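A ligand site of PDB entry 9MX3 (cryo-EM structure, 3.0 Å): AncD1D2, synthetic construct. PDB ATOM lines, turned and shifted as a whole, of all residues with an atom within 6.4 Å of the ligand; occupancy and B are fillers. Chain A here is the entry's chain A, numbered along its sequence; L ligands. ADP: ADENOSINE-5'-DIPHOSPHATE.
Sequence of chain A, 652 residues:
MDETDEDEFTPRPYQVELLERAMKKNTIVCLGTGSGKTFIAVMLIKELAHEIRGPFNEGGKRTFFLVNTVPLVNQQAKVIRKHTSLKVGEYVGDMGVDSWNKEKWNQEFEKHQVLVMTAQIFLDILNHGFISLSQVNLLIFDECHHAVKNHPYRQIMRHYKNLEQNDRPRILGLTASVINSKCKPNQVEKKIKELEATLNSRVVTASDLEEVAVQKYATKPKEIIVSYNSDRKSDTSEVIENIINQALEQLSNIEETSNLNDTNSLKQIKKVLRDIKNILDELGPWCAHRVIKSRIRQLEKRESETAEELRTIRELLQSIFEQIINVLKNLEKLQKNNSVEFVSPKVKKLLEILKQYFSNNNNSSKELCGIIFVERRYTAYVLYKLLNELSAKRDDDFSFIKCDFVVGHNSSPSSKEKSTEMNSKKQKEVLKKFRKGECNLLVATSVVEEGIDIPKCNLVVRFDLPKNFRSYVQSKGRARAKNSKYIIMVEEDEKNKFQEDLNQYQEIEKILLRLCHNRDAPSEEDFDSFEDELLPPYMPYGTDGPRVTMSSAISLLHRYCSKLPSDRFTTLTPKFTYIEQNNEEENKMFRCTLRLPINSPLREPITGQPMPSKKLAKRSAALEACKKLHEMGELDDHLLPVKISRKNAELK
The backbone NH (N) of Lys 37 sits at hydrogen-bond distance from an oxygen (O1B) of the ligand (2.4 Å).
N of Gly 34 sits at hydrogen-bond distance from O3B of the ligand.
NE2 of Gln 15 is in hydrogen-bond range of N1 of the ligand, 2.7 Å away.
The backbone NH (N) of Thr 38 is in hydrogen-bond range of an oxygen (O1B) of the ligand, at 3.4 Å.
The side-chain hydroxyl of Thr 38 is in hydrogen-bond range of an oxygen (O2A) of the ligand.
The backbone NH of Ser 35 lies within hydrogen-bond range of an oxygen (O3B) of the ligand (3.0 Å).
The guanidinium group (NE) of Arg 12 is in hydrogen-bond range of a nitrogen (N1) of the ligand (3.0 Å).
The backbone carbonyl oxygen (O) of Glu 8 is in hydrogen-bond range of a nitrogen (N6) of the ligand, at 3.3 Å.
The backbone NH (N) of Gly 36 lies close to an oxygen (O1B) of the ligand.
A nitrogen (N3) of the ligand sits close to the side-chain amino group (NZ) of Lys 216 (3.5 Å).
O of Gly 32 sits close to O3B of the ligand (3.4 Å).
Residues that only touch the ligand: Thr 10 (3.7 Å), Pro 11 (3.9 Å), Thr 33 (3.3 Å) and Phe 39 (3.4 Å).
Hydrophobic or aromatic side chains within 4 Å of the ligand: Phe 39.
Within 4 Å of the ligand: Glu 8, Thr 10, Pro 11, Arg 12, Gln 15, Gly 32, Thr 33, Gly 34, Ser 35, Gly 36, Lys 37, Thr 38, Phe 39 and Lys 216.
The side-chain amino group (NZ) of Lys 37 is in hydrogen-bond range of the backbone carbonyl oxygen (O) of Leu 31, 3.1 Å away.
The side-chain amide oxygen (OE1) of Gln 15 lies within hydrogen-bond range of the backbone NH (N) of Arg 12 (2.9 Å).
O of Ser 35 lies within hydrogen-bond range of NZ of Lys 216 (2.5 Å).
The side-chain hydroxyl of Ser 35 is in hydrogen-bond range of the backbone carbonyl oxygen of Gly 32 (2.9 Å).
The guanidinium group (NE) of Arg 12 is in salt-bridge range of the side-chain carboxylate (OE1) of Glu 8 (2.8 Å).
The guanidinium group (NH2) of Arg 12 lies within hydrogen-bond range of the side-chain amide oxygen (OE1) of Gln 215, at 3.3 Å.
The side-chain amino group (NZ) of Lys 216 is in hydrogen-bond range of the side-chain hydroxyl (OH) of Tyr 14, at 2.8 Å.
The backbone carbonyl oxygen (O) of Gly 32 lies within hydrogen-bond range of the side-chain hydroxyl (OH) of Tyr 217 (2.9 Å).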
ATOM      1  N   GLU A   6     -28.572  33.316 -35.416  1.00  0.00           N
ATOM      2  CA  GLU A   6     -28.905  31.930 -35.700  1.00  0.00           C
ATOM      3  C   GLU A   6     -28.588  31.037 -34.500  1.00  0.00           C
ATOM      4  O   GLU A   6     -27.529  31.148 -33.893  1.00  0.00           O
ATOM      5  CB  GLU A   6     -28.134  31.429 -36.924  1.00  0.00           C
ATOM      6  CG  GLU A   6     -28.063  29.918 -37.032  1.00  0.00           C
ATOM      7  CD  GLU A   6     -26.700  29.428 -37.492  1.00  0.00           C
ATOM      8  OE1 GLU A   6     -26.438  28.211 -37.365  1.00  0.00           O
ATOM      9  OE2 GLU A   6     -25.905  30.248 -37.982  1.00  0.00           O
ATOM     10  N   ASP A   7     -29.524  30.155 -34.168  1.00  0.00           N
ATOM     11  CA  ASP A   7     -29.342  29.197 -33.081  1.00  0.00           C
ATOM     12  C   ASP A   7     -28.754  27.908 -33.624  1.00  0.00           C
ATOM     13  O   ASP A   7     -28.779  27.643 -34.832  1.00  0.00           O
ATOM     14  CB  ASP A   7     -30.676  28.910 -32.372  1.00  0.00           C
ATOM     15  CG  ASP A   7     -31.670  28.213 -33.272  1.00  0.00           C
ATOM     16  OD1 ASP A   7     -31.620  26.970 -33.375  1.00  0.00           O
ATOM     17  OD2 ASP A   7     -32.521  28.912 -33.873  1.00  0.00           O
ATOM     18  N   GLU A   8     -28.228  27.089 -32.711  1.00  0.00           N
ATOM     19  CA  GLU A   8     -27.655  25.792 -33.066  1.00  0.00           C
ATOM     20  C   GLU A   8     -28.809  24.855 -33.374  1.00  0.00           C
ATOM     21  O   GLU A   8     -29.345  24.164 -32.502  1.00  0.00           O
ATOM     22  CB  GLU A   8     -26.777  25.269 -31.932  1.00  0.00           C
ATOM     23  CG  GLU A   8     -25.668  26.207 -31.508  1.00  0.00           C
ATOM     24  CD  GLU A   8     -24.688  25.555 -30.554  1.00  0.00           C
ATOM     25  OE1 GLU A   8     -24.621  24.306 -30.534  1.00  0.00           O
ATOM     26  OE2 GLU A   8     -23.991  26.272 -29.819  1.00  0.00           O
ATOM     27  N   PHE A   9     -29.197  24.822 -34.650  1.00  0.00           N
ATOM     28  CA  PHE A   9     -30.332  24.005 -35.078  1.00  0.00           C
ATOM     29  C   PHE A   9     -30.143  22.545 -34.685  1.00  0.00           C
ATOM     30  O   PHE A   9     -31.095  21.882 -34.250  1.00  0.00           O
ATOM     31  CB  PHE A   9     -30.528  24.135 -36.594  1.00  0.00           C
ATOM     32  CG  PHE A   9     -30.696  25.557 -37.061  1.00  0.00           C
ATOM     33  CD1 PHE A   9     -31.711  26.347 -36.555  1.00  0.00           C
ATOM     34  CD2 PHE A   9     -29.851  26.086 -38.014  1.00  0.00           C
ATOM     35  CE1 PHE A   9     -31.879  27.645 -36.992  1.00  0.00           C
ATOM     36  CE2 PHE A   9     -30.009  27.376 -38.458  1.00  0.00           C
ATOM     37  CZ  PHE A   9     -31.022  28.168 -37.939  1.00  0.00           C
ATOM     38  N   THR A  10     -28.940  22.040 -34.843  1.00  0.00           N
ATOM     39  CA  THR A  10     -28.667  20.661 -34.473  1.00  0.00           C
ATOM     40  C   THR A  10     -28.434  20.560 -32.969  1.00  0.00           C
ATOM     41  O   THR A  10     -27.462  21.147 -32.480  1.00  0.00           O
ATOM     42  CB  THR A  10     -27.456  20.126 -35.233  1.00  0.00           C
ATOM     43  OG1 THR A  10     -26.320  20.957 -34.941  1.00  0.00           O
ATOM     44  CG2 THR A  10     -27.714  20.149 -36.723  1.00  0.00           C
ATOM     45  N   PRO A  11     -29.269  19.862 -32.218  1.00  0.00           N
ATOM     46  CA  PRO A  11     -29.023  19.710 -30.784  1.00  0.00           C
ATOM     47  C   PRO A  11     -27.864  18.773 -30.524  1.00  0.00           C
ATOM     48  O   PRO A  11     -27.534  17.892 -31.330  1.00  0.00           O
ATOM     49  CB  PRO A  11     -30.337  19.138 -30.243  1.00  0.00           C
ATOM     50  CG  PRO A  11     -31.329  19.276 -31.373  1.00  0.00           C
ATOM     51  CD  PRO A  11     -30.531  19.228 -32.629  1.00  0.00           C
ATOM     52  N   ARG A  12     -27.229  18.961 -29.383  1.00  0.00           N
ATOM     53  CA  ARG A  12     -26.188  18.057 -28.940  1.00  0.00           C
ATOM     54  C   ARG A  12     -26.803  16.778 -28.386  1.00  0.00           C
ATOM     55  O   ARG A  12     -27.942  16.776 -27.924  1.00  0.00           O
ATOM     56  CB  ARG A  12     -25.331  18.734 -27.865  1.00  0.00           C
ATOM     57  CG  ARG A  12     -25.229  20.236 -28.041  1.00  0.00           C
ATOM     58  CD  ARG A  12     -24.291  20.591 -29.177  1.00  0.00           C
ATOM     59  NE  ARG A  12     -23.847  21.978 -29.113  1.00  0.00           N
ATOM     60  CZ  ARG A  12     -22.851  22.410 -28.356  1.00  0.00           C
ATOM     61  NH1 ARG A  12     -22.188  21.592 -27.548  1.00  0.00           N
ATOM     62  NH2 ARG A  12     -22.509  23.692 -28.400  1.00  0.00           N
ATOM     63  N   TYR A  14     -26.448  15.042 -25.647  1.00  0.00           N
ATOM     64  CA  TYR A  14     -26.906  15.085 -24.272  1.00  0.00           C
ATOM     65  C   TYR A  14     -28.185  15.908 -24.130  1.00  0.00           C
ATOM     66  O   TYR A  14     -29.025  15.602 -23.288  1.00  0.00           O
ATOM     67  CB  TYR A  14     -25.811  15.613 -23.352  1.00  0.00           C
ATOM     68  CG  TYR A  14     -25.409  17.047 -23.572  1.00  0.00           C
ATOM     69  CD1 TYR A  14     -26.027  18.080 -22.898  1.00  0.00           C
ATOM     70  CD2 TYR A  14     -24.385  17.369 -24.470  1.00  0.00           C
ATOM     71  CE1 TYR A  14     -25.647  19.395 -23.095  1.00  0.00           C
ATOM     72  CE2 TYR A  14     -24.005  18.676 -24.672  1.00  0.00           C
ATOM     73  CZ  TYR A  14     -24.642  19.680 -23.988  1.00  0.00           C
ATOM     74  OH  TYR A  14     -24.263  20.992 -24.198  1.00  0.00           O
ATOM     75  N   GLN A  15     -28.345  16.942 -24.958  1.00  0.00           N
ATOM     76  CA  GLN A  15     -29.591  17.691 -24.964  1.00  0.00           C
ATOM     77  C   GLN A  15     -30.760  16.797 -25.361  1.00  0.00           C
ATOM     78  O   GLN A  15     -31.829  16.843 -24.751  1.00  0.00           O
ATOM     79  CB  GLN A  15     -29.492  18.892 -25.910  1.00  0.00           C
ATOM     80  CG  GLN A  15     -28.412  19.883 -25.532  1.00  0.00           C
ATOM     81  CD  GLN A  15     -28.231  20.957 -26.583  1.00  0.00           C
ATOM     82  OE1 GLN A  15     -28.656  20.798 -27.729  1.00  0.00           O
ATOM     83  NE2 GLN A  15     -27.590  22.052 -26.210  1.00  0.00           N
ATOM     84  N   LEU A  31     -27.252  21.804 -14.394  1.00  0.00           N
ATOM     85  CA  LEU A  31     -26.133  21.977 -15.305  1.00  0.00           C
ATOM     86  C   LEU A  31     -25.478  23.325 -15.039  1.00  0.00           C
ATOM     87  O   LEU A  31     -26.085  24.233 -14.468  1.00  0.00           O
ATOM     88  CB  LEU A  31     -26.584  21.874 -16.769  1.00  0.00           C
ATOM     89  CG  LEU A  31     -26.571  20.486 -17.397  1.00  0.00           C
ATOM     90  CD1 LEU A  31     -27.172  20.540 -18.799  1.00  0.00           C
ATOM     91  CD2 LEU A  31     -25.167  19.922 -17.435  1.00  0.00           C
ATOM     92  N   GLY A  32     -24.229  23.444 -15.470  1.00  0.00           N
ATOM     93  CA  GLY A  32     -23.509  24.690 -15.349  1.00  0.00           C
ATOM     94  C   GLY A  32     -23.949  25.716 -16.374  1.00  0.00           C
ATOM     95  O   GLY A  32     -24.645  25.411 -17.340  1.00  0.00           O
ATOM     96  N   THR A  33     -23.527  26.957 -16.148  1.00  0.00           N
ATOM     97  CA  THR A  33     -23.938  28.050 -17.017  1.00  0.00           C
ATOM     98  C   THR A  33     -23.398  27.843 -18.437  1.00  0.00           C
ATOM     99  O   THR A  33     -22.301  27.329 -18.630  1.00  0.00           O
ATOM    100  CB  THR A  33     -23.445  29.384 -16.470  1.00  0.00           C
ATOM    101  OG1 THR A  33     -22.041  29.304 -16.206  1.00  0.00           O
ATOM    102  CG2 THR A  33     -24.169  29.723 -15.176  1.00  0.00           C
ATOM    103  N   GLY A  34     -24.199  28.247 -19.420  1.00  0.00           N
ATOM    104  CA  GLY A  34     -23.840  28.091 -20.814  1.00  0.00           C
ATOM    105  C   GLY A  34     -24.156  26.738 -21.401  1.00  0.00           C
ATOM    106  O   GLY A  34     -23.962  26.555 -22.606  1.00  0.00           O
ATOM    107  N   SER A  35     -24.639  25.790 -20.591  1.00  0.00           N
ATOM    108  CA  SER A  35     -24.990  24.481 -21.133  1.00  0.00           C
ATOM    109  C   SER A  35     -26.178  24.579 -22.088  1.00  0.00           C
ATOM    110  O   SER A  35     -26.261  23.831 -23.063  1.00  0.00           O
ATOM    111  CB  SER A  35     -25.295  23.513 -19.996  1.00  0.00           C
ATOM    112  OG  SER A  35     -26.356  23.998 -19.185  1.00  0.00           O
ATOM    113  N   GLY A  36     -27.108  25.490 -21.807  1.00  0.00           N
ATOM    114  CA  GLY A  36     -28.241  25.695 -22.692  1.00  0.00           C
ATOM    115  C   GLY A  36     -29.557  25.176 -22.142  1.00  0.00           C
ATOM    116  O   GLY A  36     -30.364  24.623 -22.888  1.00  0.00           O
ATOM    117  N   LYS A  37     -29.777  25.345 -20.835  1.00  0.00           N
ATOM    118  CA  LYS A  37     -31.016  24.882 -20.228  1.00  0.00           C
ATOM    119  C   LYS A  37     -32.230  25.578 -20.818  1.00  0.00           C
ATOM    120  O   LYS A  37     -33.302  24.972 -20.945  1.00  0.00           O
ATOM    121  CB  LYS A  37     -30.965  25.075 -18.712  1.00  0.00           C
ATOM    122  CG  LYS A  37     -29.857  24.273 -18.039  1.00  0.00           C
ATOM    123  CD  LYS A  37     -29.731  24.649 -16.577  1.00  0.00           C
ATOM    124  CE  LYS A  37     -29.090  26.010 -16.408  1.00  0.00           C
ATOM    125  NZ  LYS A  37     -28.445  26.148 -15.073  1.00  0.00           N
ATOM    126  N   THR A  38     -32.085  26.848 -21.193  1.00  0.00           N
ATOM    127  CA  THR A  38     -33.176  27.562 -21.841  1.00  0.00           C
ATOM    128  C   THR A  38     -33.553  26.909 -23.160  1.00  0.00           C
ATOM    129  O   THR A  38     -34.748  26.814 -23.496  1.00  0.00           O
ATOM    130  CB  THR A  38     -32.786  29.024 -22.066  1.00  0.00           C
ATOM    131  OG1 THR A  38     -32.426  29.616 -20.818  1.00  0.00           O
ATOM    132  CG2 THR A  38     -33.944  29.795 -22.667  1.00  0.00           C
ATOM    133  N   PHE A  39     -32.566  26.431 -23.919  1.00  0.00           N
ATOM    134  CA  PHE A  39     -32.850  25.729 -25.165  1.00  0.00           C
ATOM    135  C   PHE A  39     -33.627  24.450 -24.904  1.00  0.00           C
ATOM    136  O   PHE A  39     -34.545  24.105 -25.656  1.00  0.00           O
ATOM    137  CB  PHE A  39     -31.556  25.438 -25.906  1.00  0.00           C
ATOM    138  CG  PHE A  39     -31.650  25.688 -27.376  1.00  0.00           C
ATOM    139  CD1 PHE A  39     -32.153  26.886 -27.856  1.00  0.00           C
ATOM    140  CD2 PHE A  39     -31.240  24.730 -28.290  1.00  0.00           C
ATOM    141  CE1 PHE A  39     -32.241  27.118 -29.219  1.00  0.00           C
ATOM    142  CE2 PHE A  39     -31.327  24.957 -29.645  1.00  0.00           C
ATOM    143  CZ  PHE A  39     -31.828  26.149 -30.117  1.00  0.00           C
ATOM    144  N   HIS A  83     -37.221  31.756 -31.167  1.00  0.00           N
ATOM    145  CA  HIS A  83     -36.927  30.365 -31.523  1.00  0.00           C
ATOM    146  C   HIS A  83     -38.125  29.621 -32.085  1.00  0.00           C
ATOM    147  O   HIS A  83     -37.946  28.659 -32.844  1.00  0.00           O
ATOM    148  CB  HIS A  83     -36.373  29.622 -30.317  1.00  0.00           C
ATOM    149  CG  HIS A  83     -34.915  29.878 -30.067  1.00  0.00           C
ATOM    150  ND1 HIS A  83     -34.454  30.435 -28.904  1.00  0.00           N
ATOM    151  CD2 HIS A  83     -33.833  29.669 -30.852  1.00  0.00           C
ATOM    152  CE1 HIS A  83     -33.134  30.549 -28.969  1.00  0.00           C
ATOM    153  NE2 HIS A  83     -32.743  30.104 -30.144  1.00  0.00           N
ATOM    154  N   GLN A 215     -16.767  20.544 -24.497  1.00  0.00           N
ATOM    155  CA  GLN A 215     -17.278  21.487 -25.478  1.00  0.00           C
ATOM    156  C   GLN A 215     -17.296  22.911 -24.946  1.00  0.00           C
ATOM    157  O   GLN A 215     -16.835  23.838 -25.624  1.00  0.00           O
ATOM    158  CB  GLN A 215     -18.685  21.067 -25.922  1.00  0.00           C
ATOM    159  CG  GLN A 215     -18.907  21.164 -27.419  1.00  0.00           C
ATOM    160  CD  GLN A 215     -19.283  22.560 -27.868  1.00  0.00           C
ATOM    161  OE1 GLN A 215     -19.522  23.451 -27.047  1.00  0.00           O
ATOM    162  NE2 GLN A 215     -19.353  22.769 -29.177  1.00  0.00           N
ATOM    163  N   LYS A 216     -17.804  23.115 -23.735  1.00  0.00           N
ATOM    164  CA  LYS A 216     -18.042  24.448 -23.211  1.00  0.00           C
ATOM    165  C   LYS A 216     -17.207  24.767 -21.974  1.00  0.00           C
ATOM    166  O   LYS A 216     -16.540  25.809 -21.936  1.00  0.00           O
ATOM    167  CB  LYS A 216     -19.532  24.633 -22.896  1.00  0.00           C
ATOM    168  CG  LYS A 216     -20.440  24.337 -24.071  1.00  0.00           C
ATOM    169  CD  LYS A 216     -21.877  24.171 -23.627  1.00  0.00           C
ATOM    170  CE  LYS A 216     -22.787  23.872 -24.816  1.00  0.00           C
ATOM    171  NZ  LYS A 216     -24.214  23.813 -24.414  1.00  0.00           N
ATOM    172  N   TYR A 217     -17.221  23.900 -20.965  1.00  0.00           N
ATOM    173  CA  TYR A 217     -16.513  24.161 -19.718  1.00  0.00           C
ATOM    174  C   TYR A 217     -15.008  23.999 -19.843  1.00  0.00           C
ATOM    175  O   TYR A 217     -14.312  24.055 -18.818  1.00  0.00           O
ATOM    176  CB  TYR A 217     -17.058  23.255 -18.610  1.00  0.00           C
ATOM    177  CG  TYR A 217     -18.565  23.290 -18.469  1.00  0.00           C
ATOM    178  CD1 TYR A 217     -19.255  24.494 -18.545  1.00  0.00           C
ATOM    179  CD2 TYR A 217     -19.284  22.134 -18.260  1.00  0.00           C
ATOM    180  CE1 TYR A 217     -20.633  24.529 -18.413  1.00  0.00           C
ATOM    181  CE2 TYR A 217     -20.661  22.156 -18.125  1.00  0.00           C
ATOM    182  CZ  TYR A 217     -21.331  23.360 -18.204  1.00  0.00           C
ATOM    183  OH  TYR A 217     -22.699  23.396 -18.073  1.00  0.00           O
ATOM    184  N   ASP A 453     -27.851  38.761 -18.253  1.00  0.00           N
ATOM    185  CA  ASP A 453     -26.945  38.520 -19.374  1.00  0.00           C
ATOM    186  C   ASP A 453     -25.800  39.521 -19.322  1.00  0.00           C
ATOM    187  O   ASP A 453     -26.027  40.727 -19.414  1.00  0.00           O
ATOM    188  CB  ASP A 453     -27.689  38.625 -20.696  1.00  0.00           C
ATOM    189  CG  ASP A 453     -26.852  38.171 -21.867  1.00  0.00           C
ATOM    190  OD1 ASP A 453     -25.860  37.453 -21.646  1.00  0.00           O
ATOM    191  OD2 ASP A 453     -27.189  38.528 -23.017  1.00  0.00           O
HETATM  192  PB  ADP L   1     -27.789  28.329 -19.558  1.00  0.00           P
HETATM  193  O1B ADP L   1     -28.861  27.475 -20.197  1.00  0.00           O
HETATM  194  O2B ADP L   1     -28.306  29.305 -18.531  1.00  0.00           O
HETATM  195  O3B ADP L   1     -26.565  27.559 -19.134  1.00  0.00           O
HETATM  196  PA  ADP L   1     -28.216  30.308 -21.503  1.00  0.00           P
HETATM  197  O1A ADP L   1     -27.999  31.664 -20.897  1.00  0.00           O
HETATM  198  O2A ADP L   1     -29.611  29.729 -21.536  1.00  0.00           O
HETATM  199  O3A ADP L   1     -27.246  29.278 -20.735  1.00  0.00           O
HETATM  200  O5' ADP L   1     -27.617  30.344 -22.996  1.00  0.00           O
HETATM  201  C5' ADP L   1     -27.284  29.136 -23.672  1.00  0.00           C
HETATM  202  C4' ADP L   1     -26.415  29.485 -24.871  1.00  0.00           C
HETATM  203  O4' ADP L   1     -26.125  28.315 -25.624  1.00  0.00           O
HETATM  204  C3' ADP L   1     -27.122  30.462 -25.799  1.00  0.00           C
HETATM  205  O3' ADP L   1     -26.517  31.747 -25.695  1.00  0.00           O
HETATM  206  C2' ADP L   1     -26.938  29.914 -27.194  1.00  0.00           C
HETATM  207  O2' ADP L   1     -26.179  30.829 -27.987  1.00  0.00           O
HETATM  208  C1' ADP L   1     -26.171  28.615 -27.024  1.00  0.00           C
HETATM  209  N9  ADP L   1     -26.852  27.521 -27.758  1.00  0.00           N
HETATM  210  C8  ADP L   1     -27.920  27.653 -28.569  1.00  0.00           C
HETATM  211  N7  ADP L   1     -28.294  26.463 -29.092  1.00  0.00           N
HETATM  212  C5  ADP L   1     -27.439  25.533 -28.612  1.00  0.00           C
HETATM  213  C6  ADP L   1     -27.277  24.066 -28.779  1.00  0.00           C
HETATM  214  N6  ADP L   1     -28.103  23.350 -29.563  1.00  0.00           N
HETATM  215  N1  ADP L   1     -26.259  23.482 -28.110  1.00  0.00           N
HETATM  216  C2  ADP L   1     -25.424  24.191 -27.332  1.00  0.00           C
HETATM  217  N3  ADP L   1     -25.525  25.517 -27.132  1.00  0.00           N
HETATM  218  C4  ADP L   1     -26.491  26.232 -27.751  1.00  0.00           C
